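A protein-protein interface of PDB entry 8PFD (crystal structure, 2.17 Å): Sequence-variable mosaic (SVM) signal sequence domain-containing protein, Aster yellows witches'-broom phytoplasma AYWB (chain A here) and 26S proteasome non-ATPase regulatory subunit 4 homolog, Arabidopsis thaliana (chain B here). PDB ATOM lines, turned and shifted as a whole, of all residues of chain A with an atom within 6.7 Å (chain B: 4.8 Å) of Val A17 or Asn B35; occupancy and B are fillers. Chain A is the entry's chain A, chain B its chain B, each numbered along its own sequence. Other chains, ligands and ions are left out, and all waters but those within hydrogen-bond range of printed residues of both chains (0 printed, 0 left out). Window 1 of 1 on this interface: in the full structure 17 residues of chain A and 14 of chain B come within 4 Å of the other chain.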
ATOM      1  N   VAL A  15      20.265 -35.662 -29.582  1.00  0.00           N
ATOM      2  CA  VAL A  15      19.040 -35.582 -28.746  1.00  0.00           C
ATOM      3  C   VAL A  15      17.996 -34.764 -29.510  1.00  0.00           C
ATOM      4  O   VAL A  15      18.010 -33.514 -29.394  1.00  0.00           O
ATOM      5  CB  VAL A  15      19.351 -34.976 -27.361  1.00  0.00           C
ATOM      6  CG1 VAL A  15      18.134 -35.069 -26.449  1.00  0.00           C
ATOM      7  CG2 VAL A  15      20.563 -35.622 -26.709  1.00  0.00           C
ATOM      8  N   ASN A  16      17.098 -35.446 -30.214  1.00  0.00           N
ATOM      9  CA  ASN A  16      15.944 -34.815 -30.922  1.00  0.00           C
ATOM     10  C   ASN A  16      14.907 -34.390 -29.887  1.00  0.00           C
ATOM     11  O   ASN A  16      14.440 -35.252 -29.119  1.00  0.00           O
ATOM     12  CB  ASN A  16      15.334 -35.754 -31.963  1.00  0.00           C
ATOM     13  CG  ASN A  16      16.353 -36.089 -33.031  1.00  0.00           C
ATOM     14  OD1 ASN A  16      16.695 -35.257 -33.862  1.00  0.00           O
ATOM     15  ND2 ASN A  16      16.933 -37.266 -32.952  1.00  0.00           N
ATOM     16  N   VAL A  17      14.601 -33.097 -29.866  1.00  0.00           N
ATOM     17  CA  VAL A  17      13.576 -32.474 -28.984  1.00  0.00           C
ATOM     18  C   VAL A  17      12.550 -31.793 -29.887  1.00  0.00           C
ATOM     19  O   VAL A  17      12.941 -30.931 -30.690  1.00  0.00           O
ATOM     20  CB  VAL A  17      14.216 -31.485 -27.994  1.00  0.00           C
ATOM     21  CG1 VAL A  17      13.266 -31.155 -26.865  1.00  0.00           C
ATOM     22  CG2 VAL A  17      15.533 -32.013 -27.440  1.00  0.00           C
ATOM     23  N   ASN A  18      11.297 -32.204 -29.746  1.00  0.00           N
ATOM     24  CA  ASN A  18      10.122 -31.673 -30.471  1.00  0.00           C
ATOM     25  C   ASN A  18       9.409 -30.674 -29.555  1.00  0.00           C
ATOM     26  O   ASN A  18       9.084 -31.054 -28.425  1.00  0.00           O
ATOM     27  CB  ASN A  18       9.160 -32.787 -30.883  1.00  0.00           C
ATOM     28  CG  ASN A  18       9.811 -33.925 -31.640  1.00  0.00           C
ATOM     29  OD1 ASN A  18      10.745 -33.740 -32.415  1.00  0.00           O
ATOM     30  ND2 ASN A  18       9.280 -35.117 -31.443  1.00  0.00           N
ATOM     31  N   LEU A  19       9.180 -29.452 -30.037  1.00  0.00           N
ATOM     32  CA  LEU A  19       8.448 -28.383 -29.310  1.00  0.00           C
ATOM     33  C   LEU A  19       7.214 -27.979 -30.124  1.00  0.00           C
ATOM     34  O   LEU A  19       7.298 -27.907 -31.363  1.00  0.00           O
ATOM     35  CB  LEU A  19       9.397 -27.198 -29.108  1.00  0.00           C
ATOM     36  CG  LEU A  19      10.803 -27.561 -28.623  1.00  0.00           C
ATOM     37  CD1 LEU A  19      11.768 -26.427 -28.882  1.00  0.00           C
ATOM     38  CD2 LEU A  19      10.813 -27.929 -27.150  1.00  0.00           C
ATOM     39  N   ILE A  24       8.387 -22.253 -25.472  1.00  0.00           N
ATOM     40  CA  ILE A  24       8.535 -23.262 -24.375  1.00  0.00           C
ATOM     41  C   ILE A  24       9.927 -23.105 -23.746  1.00  0.00           C
ATOM     42  O   ILE A  24      10.042 -23.232 -22.514  1.00  0.00           O
ATOM     43  CB  ILE A  24       8.287 -24.704 -24.878  1.00  0.00           C
ATOM     44  CG1 ILE A  24       6.801 -25.068 -24.856  1.00  0.00           C
ATOM     45  CG2 ILE A  24       9.100 -25.718 -24.085  1.00  0.00           C
ATOM     46  CD1 ILE A  24       5.954 -24.297 -25.842  1.00  0.00           C
ATOM     47  N   LEU A  25      10.945 -22.817 -24.556  1.00  0.00           N
ATOM     48  CA  LEU A  25      12.363 -22.760 -24.113  1.00  0.00           C
ATOM     49  C   LEU A  25      12.653 -21.511 -23.268  1.00  0.00           C
ATOM     50  O   LEU A  25      13.700 -21.519 -22.616  1.00  0.00           O
ATOM     51  CB  LEU A  25      13.257 -22.809 -25.354  1.00  0.00           C
ATOM     52  CG  LEU A  25      13.247 -24.142 -26.105  1.00  0.00           C
ATOM     53  CD1 LEU A  25      13.887 -24.009 -27.478  1.00  0.00           C
ATOM     54  CD2 LEU A  25      13.947 -25.224 -25.305  1.00  0.00           C
ATOM     55  N   HIS A  28      12.461 -22.910 -19.890  1.00  0.00           N
ATOM     56  CA  HIS A  28      13.346 -24.085 -19.657  1.00  0.00           C
ATOM     57  C   HIS A  28      14.591 -23.613 -18.913  1.00  0.00           C
ATOM     58  O   HIS A  28      15.346 -22.839 -19.501  1.00  0.00           O
ATOM     59  CB  HIS A  28      13.696 -24.792 -20.976  1.00  0.00           C
ATOM     60  CG  HIS A  28      14.156 -26.194 -20.777  1.00  0.00           C
ATOM     61  ND1 HIS A  28      15.329 -26.506 -20.107  1.00  0.00           N
ATOM     62  CD2 HIS A  28      13.602 -27.371 -21.142  1.00  0.00           C
ATOM     63  CE1 HIS A  28      15.458 -27.817 -20.054  1.00  0.00           C
ATOM     64  NE2 HIS A  28      14.411 -28.370 -20.683  1.00  0.00           N
ATOM     65  N   THR A  30      17.320 -25.008 -18.163  1.00  0.00           N
ATOM     66  CA  THR A  30      18.553 -25.313 -18.928  1.00  0.00           C
ATOM     67  C   THR A  30      18.664 -24.373 -20.141  1.00  0.00           C
ATOM     68  O   THR A  30      19.651 -23.613 -20.220  1.00  0.00           O
ATOM     69  CB  THR A  30      18.613 -26.776 -19.377  1.00  0.00           C
ATOM     70  OG1 THR A  30      18.101 -27.594 -18.324  1.00  0.00           O
ATOM     71  CG2 THR A  30      20.019 -27.181 -19.757  1.00  0.00           C
ATOM     72  N   PHE A  31      17.706 -24.412 -21.065  1.00  0.00           N
ATOM     73  CA  PHE A  31      17.912 -23.913 -22.449  1.00  0.00           C
ATOM     74  C   PHE A  31      17.678 -22.398 -22.534  1.00  0.00           C
ATOM     75  O   PHE A  31      18.269 -21.791 -23.455  1.00  0.00           O
ATOM     76  CB  PHE A  31      17.068 -24.728 -23.429  1.00  0.00           C
ATOM     77  CG  PHE A  31      17.370 -26.208 -23.407  1.00  0.00           C
ATOM     78  CD1 PHE A  31      18.681 -26.668 -23.494  1.00  0.00           C
ATOM     79  CD2 PHE A  31      16.346 -27.141 -23.303  1.00  0.00           C
ATOM     80  CE1 PHE A  31      18.957 -28.029 -23.493  1.00  0.00           C
ATOM     81  CE2 PHE A  31      16.626 -28.497 -23.271  1.00  0.00           C
ATOM     82  CZ  PHE A  31      17.929 -28.941 -23.376  1.00  0.00           C
ATOM     83  N   LEU A  65      14.352 -25.700 -35.306  1.00  0.00           N
ATOM     84  CA  LEU A  65      14.300 -24.489 -34.448  1.00  0.00           C
ATOM     85  C   LEU A  65      15.694 -24.103 -33.927  1.00  0.00           C
ATOM     86  O   LEU A  65      15.910 -22.890 -33.661  1.00  0.00           O
ATOM     87  CB  LEU A  65      13.353 -24.765 -33.281  1.00  0.00           C
ATOM     88  CG  LEU A  65      11.886 -24.997 -33.632  1.00  0.00           C
ATOM     89  CD1 LEU A  65      11.128 -25.373 -32.371  1.00  0.00           C
ATOM     90  CD2 LEU A  65      11.264 -23.770 -34.302  1.00  0.00           C
ATOM     91  N   TYR A  97      21.739 -31.180 -28.757  1.00  0.00           N
ATOM     92  CA  TYR A  97      20.265 -31.007 -28.688  1.00  0.00           C
ATOM     93  C   TYR A  97      19.782 -30.396 -30.007  1.00  0.00           C
ATOM     94  O   TYR A  97      20.284 -29.337 -30.389  1.00  0.00           O
ATOM     95  CB  TYR A  97      19.881 -30.140 -27.495  1.00  0.00           C
ATOM     96  CG  TYR A  97      20.255 -30.714 -26.155  1.00  0.00           C
ATOM     97  CD1 TYR A  97      19.382 -31.548 -25.482  1.00  0.00           C
ATOM     98  CD2 TYR A  97      21.463 -30.413 -25.545  1.00  0.00           C
ATOM     99  CE1 TYR A  97      19.686 -32.065 -24.239  1.00  0.00           C
ATOM    100  CE2 TYR A  97      21.785 -30.919 -24.290  1.00  0.00           C
ATOM    101  CZ  TYR A  97      20.890 -31.747 -23.639  1.00  0.00           C
ATOM    102  OH  TYR A  97      21.164 -32.281 -22.417  1.00  0.00           O
ATOM    103  N   ILE A  98      18.869 -31.070 -30.697  1.00  0.00           N
ATOM    104  CA  ILE A  98      18.285 -30.595 -31.989  1.00  0.00           C
ATOM    105  C   ILE A  98      16.802 -30.347 -31.736  1.00  0.00           C
ATOM    106  O   ILE A  98      16.068 -31.314 -31.518  1.00  0.00           O
ATOM    107  CB  ILE A  98      18.508 -31.587 -33.154  1.00  0.00           C
ATOM    108  CG1 ILE A  98      19.976 -31.989 -33.318  1.00  0.00           C
ATOM    109  CG2 ILE A  98      17.953 -31.020 -34.465  1.00  0.00           C
ATOM    110  CD1 ILE A  98      20.192 -33.067 -34.370  1.00  0.00           C
ATOM    111  N   PHE A  99      16.406 -29.079 -31.744  1.00  0.00           N
ATOM    112  CA  PHE A  99      15.024 -28.619 -31.464  1.00  0.00           C
ATOM    113  C   PHE A  99      14.204 -28.565 -32.751  1.00  0.00           C
ATOM    114  O   PHE A  99      14.603 -27.885 -33.698  1.00  0.00           O
ATOM    115  CB  PHE A  99      15.098 -27.265 -30.769  1.00  0.00           C
ATOM    116  CG  PHE A  99      15.876 -27.351 -29.482  1.00  0.00           C
ATOM    117  CD1 PHE A  99      15.325 -27.963 -28.370  1.00  0.00           C
ATOM    118  CD2 PHE A  99      17.178 -26.879 -29.405  1.00  0.00           C
ATOM    119  CE1 PHE A  99      16.053 -28.072 -27.195  1.00  0.00           C
ATOM    120  CE2 PHE A  99      17.892 -26.969 -28.225  1.00  0.00           C
ATOM    121  CZ  PHE A  99      17.333 -27.569 -27.124  1.00  0.00           C
ATOM    122  N   TRP A 100      13.062 -29.245 -32.738  1.00  0.00           N
ATOM    123  CA  TRP A 100      12.136 -29.382 -33.884  1.00  0.00           C
ATOM    124  C   TRP A 100      10.777 -28.794 -33.511  1.00  0.00           C
ATOM    125  O   TRP A 100      10.353 -28.976 -32.349  1.00  0.00           O
ATOM    126  CB  TRP A 100      11.975 -30.853 -34.291  1.00  0.00           C
ATOM    127  CG  TRP A 100      13.231 -31.530 -34.740  1.00  0.00           C
ATOM    128  CD1 TRP A 100      13.996 -32.401 -34.021  1.00  0.00           C
ATOM    129  CD2 TRP A 100      13.858 -31.410 -36.029  1.00  0.00           C
ATOM    130  NE1 TRP A 100      15.065 -32.817 -34.770  1.00  0.00           N
ATOM    131  CE2 TRP A 100      15.002 -32.234 -36.008  1.00  0.00           C
ATOM    132  CE3 TRP A 100      13.564 -30.688 -37.193  1.00  0.00           C
ATOM    133  CZ2 TRP A 100      15.852 -32.356 -37.107  1.00  0.00           C
ATOM    134  CZ3 TRP A 100      14.405 -30.805 -38.275  1.00  0.00           C
ATOM    135  CH2 TRP A 100      15.530 -31.632 -38.234  1.00  0.00           C
ATOM    136  N   GLN A 101      10.134 -28.144 -34.485  1.00  0.00           N
ATOM    137  CA  GLN A 101       8.678 -27.866 -34.520  1.00  0.00           C
ATOM    138  C   GLN A 101       7.895 -29.178 -34.666  1.00  0.00           C
ATOM    139  O   GLN A 101       8.153 -29.919 -35.630  1.00  0.00           O
ATOM    140  CB  GLN A 101       8.395 -26.968 -35.720  1.00  0.00           C
ATOM    141  CG  GLN A 101       6.978 -26.444 -35.765  1.00  0.00           C
ATOM    142  CD  GLN A 101       6.842 -25.349 -34.743  1.00  0.00           C
ATOM    143  OE1 GLN A 101       7.493 -24.311 -34.846  1.00  0.00           O
ATOM    144  NE2 GLN A 101       6.022 -25.595 -33.735  1.00  0.00           N
ATOM    145  N   THR B  31       5.119 -34.836 -22.635  1.00  0.00           N
ATOM    146  CA  THR B  31       6.545 -34.767 -23.077  1.00  0.00           C
ATOM    147  C   THR B  31       7.152 -33.373 -22.834  1.00  0.00           C
ATOM    148  O   THR B  31       8.294 -33.307 -22.311  1.00  0.00           O
ATOM    149  CB  THR B  31       6.657 -35.134 -24.564  1.00  0.00           C
ATOM    150  OG1 THR B  31       6.195 -36.477 -24.722  1.00  0.00           O
ATOM    151  CG2 THR B  31       8.062 -34.994 -25.108  1.00  0.00           C
ATOM    152  N   GLU B  32       6.439 -32.300 -23.210  1.00  0.00           N
ATOM    153  CA  GLU B  32       6.906 -30.891 -23.030  1.00  0.00           C
ATOM    154  C   GLU B  32       7.041 -30.556 -21.536  1.00  0.00           C
ATOM    155  O   GLU B  32       8.069 -29.941 -21.158  1.00  0.00           O
ATOM    156  CB  GLU B  32       5.978 -29.886 -23.716  1.00  0.00           C
ATOM    157  CG  GLU B  32       6.432 -29.545 -25.116  1.00  0.00           C
ATOM    158  CD  GLU B  32       5.419 -28.803 -25.978  1.00  0.00           C
ATOM    159  OE1 GLU B  32       4.205 -28.951 -25.731  1.00  0.00           O
ATOM    160  OE2 GLU B  32       5.847 -28.088 -26.914  1.00  0.00           O
ATOM    161  N   ALA B  33       6.035 -30.909 -20.730  1.00  0.00           N
ATOM    162  CA  ALA B  33       6.020 -30.675 -19.268  1.00  0.00           C
ATOM    163  C   ALA B  33       7.175 -31.460 -18.628  1.00  0.00           C
ATOM    164  O   ALA B  33       7.943 -30.889 -17.821  1.00  0.00           O
ATOM    165  CB  ALA B  33       4.671 -31.054 -18.702  1.00  0.00           C
ATOM    166  N   VAL B  34       7.340 -32.721 -19.027  1.00  0.00           N
ATOM    167  CA  VAL B  34       8.425 -33.613 -18.520  1.00  0.00           C
ATOM    168  C   VAL B  34       9.780 -32.991 -18.860  1.00  0.00           C
ATOM    169  O   VAL B  34      10.687 -33.000 -17.988  1.00  0.00           O
ATOM    170  CB  VAL B  34       8.296 -35.023 -19.107  1.00  0.00           C
ATOM    171  CG1 VAL B  34       9.503 -35.881 -18.776  1.00  0.00           C
ATOM    172  CG2 VAL B  34       6.996 -35.686 -18.669  1.00  0.00           C
ATOM    173  N   ASN B  35       9.894 -32.435 -20.066  1.00  0.00           N
ATOM    174  CA  ASN B  35      11.132 -31.776 -20.553  1.00  0.00           C
ATOM    175  C   ASN B  35      11.456 -30.555 -19.667  1.00  0.00           C
ATOM    176  O   ASN B  35      12.617 -30.420 -19.245  1.00  0.00           O
ATOM    177  CB  ASN B  35      10.982 -31.474 -22.047  1.00  0.00           C
ATOM    178  CG  ASN B  35      12.195 -30.818 -22.654  1.00  0.00           C
ATOM    179  OD1 ASN B  35      13.197 -30.610 -21.993  1.00  0.00           O
ATOM    180  ND2 ASN B  35      12.098 -30.451 -23.915  1.00  0.00           N
ATOM    181  N   LEU B  36      10.489 -29.668 -19.416  1.00  0.00           N
ATOM    182  CA  LEU B  36      10.699 -28.442 -18.593  1.00  0.00           C
ATOM    183  C   LEU B  36      11.046 -28.848 -17.155  1.00  0.00           C
ATOM    184  O   LEU B  36      11.934 -28.214 -16.566  1.00  0.00           O
ATOM    185  CB  LEU B  36       9.441 -27.569 -18.625  1.00  0.00           C
ATOM    186  CG  LEU B  36       9.268 -26.731 -19.886  1.00  0.00           C
ATOM    187  CD1 LEU B  36       7.922 -26.012 -19.870  1.00  0.00           C
ATOM    188  CD2 LEU B  36      10.410 -25.739 -20.027  1.00  0.00           C
ATOM    189  N   LEU B  37      10.363 -29.874 -16.641  1.00  0.00           N
ATOM    190  CA  LEU B  37      10.476 -30.383 -15.251  1.00  0.00           C
ATOM    191  C   LEU B  37      11.844 -31.035 -14.998  1.00  0.00           C
ATOM    192  O   LEU B  37      12.393 -30.869 -13.893  1.00  0.00           O
ATOM    193  CB  LEU B  37       9.331 -31.375 -15.058  1.00  0.00           C
ATOM    194  CG  LEU B  37       9.111 -31.921 -13.652  1.00  0.00           C
ATOM    195  CD1 LEU B  37       9.078 -30.820 -12.599  1.00  0.00           C
ATOM    196  CD2 LEU B  37       7.825 -32.740 -13.617  1.00  0.00           C
ATOM    197  N   CYS B  38      12.376 -31.774 -15.970  1.00  0.00           N
ATOM    198  CA  CYS B  38      13.730 -32.373 -15.896  1.00  0.00           C
ATOM    199  C   CYS B  38      14.755 -31.256 -15.990  1.00  0.00           C
ATOM    200  O   CYS B  38      15.833 -31.402 -15.413  1.00  0.00           O
ATOM    201  CB  CYS B  38      13.967 -33.363 -17.024  1.00  0.00           C
ATOM    202  SG  CYS B  38      12.900 -34.809 -16.893  1.00  0.00           S
ATOM    203  N   GLY B  39      14.402 -30.187 -16.704  1.00  0.00           N
ATOM    204  CA  GLY B  39      15.211 -28.962 -16.793  1.00  0.00           C
ATOM    205  C   GLY B  39      15.379 -28.349 -15.422  1.00  0.00           C
ATOM    206  O   GLY B  39      16.537 -28.243 -14.964  1.00  0.00           O
ATOM    207  N   LEU B  74      15.940 -36.876 -22.094  1.00  0.00           N
ATOM    208  CA  LEU B  74      15.080 -36.314 -23.177  1.00  0.00           C
ATOM    209  C   LEU B  74      15.111 -37.218 -24.415  1.00  0.00           C
ATOM    210  O   LEU B  74      14.055 -37.317 -25.090  1.00  0.00           O
ATOM    211  CB  LEU B  74      15.517 -34.887 -23.527  1.00  0.00           C
ATOM    212  CG  LEU B  74      15.449 -33.880 -22.387  1.00  0.00           C
ATOM    213  CD1 LEU B  74      15.733 -32.484 -22.910  1.00  0.00           C
ATOM    214  CD2 LEU B  74      14.106 -33.936 -21.679  1.00  0.00           C
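A ring nitrogen (NE2) of His A28 sits at hydrogen-bond distance from the side-chain amide oxygen of Asn B35, 2.9 Å away.
N of Ile A98 sits at hydrogen-bond distance from O of Val A15, at 2.9 Å.
N of Val A17 sits at hydrogen-bond distance from O of Ile A98 (2.8 Å).
The backbone carbonyl oxygen (O) of Val A17 lies within hydrogen-bond range of the backbone NH (N) of Trp A100.
N of Leu A19 sits at hydrogen-bond distance from O of Trp A100, at 2.6 Å.
The backbone NH (N) of Thr A30 sits close to a ring nitrogen (ND1) of His A28, at 3.2 Å.
The backbone NH of Phe A31 is in hydrogen-bond range of a ring nitrogen (ND1) of His A28 (3.3 Å).
Among the printed residues, pairs that only touch across the chains: Val A17 with Asn B35, His A28 with Leu B36, His A28 with Gly B39, Leu A19 with Glu B32, Thr A30 with Gly B39, Ile A24 with Leu B36, Ile A24 with Glu B32 and Val A15 with Leu B74.
Of chain B, only Asn B35 comes within 4 Å of Val A17.
Asn B35 touches two residues of chain A.
Printed residues of chain A within 4 Å of Glu B32: Leu A19 and Ile A24.
Of the printed residues of chain B, Ile A24 touches Glu B32 (3.8 Å) and Leu B36 (3.6 Å).
Leu A25 touches none of the printed residues of chain B.
Val B34 touches none of the printed residues of chain A.
The nearest residue of chain B that does not touch Val A17 is Leu B74 (4.6 Å).
Of the 10 printed residues of chain B, 5 touch a printed residue of chain A.
Hydrophobic or aromatic side chains of chain B that line the printed part of chain A: Leu B36 and Leu B74.
Of the 16 printed residues of chain A, 6 touch a printed residue of chain B.
Printed residues of chain A that touch a printed residue of chain B: Val A15, Val A17, Leu A19, Ile A24, His A28 and Thr A30.
Hydrophobic or aromatic side chains of chain A that line the printed part of chain B: Val A15, Val A17, Ile A24 and His A28.
Among the printed residues, no Asp or Glu carboxylate lies within 4 Å of a Lys or Arg side-chain nitrogen of the other chain.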
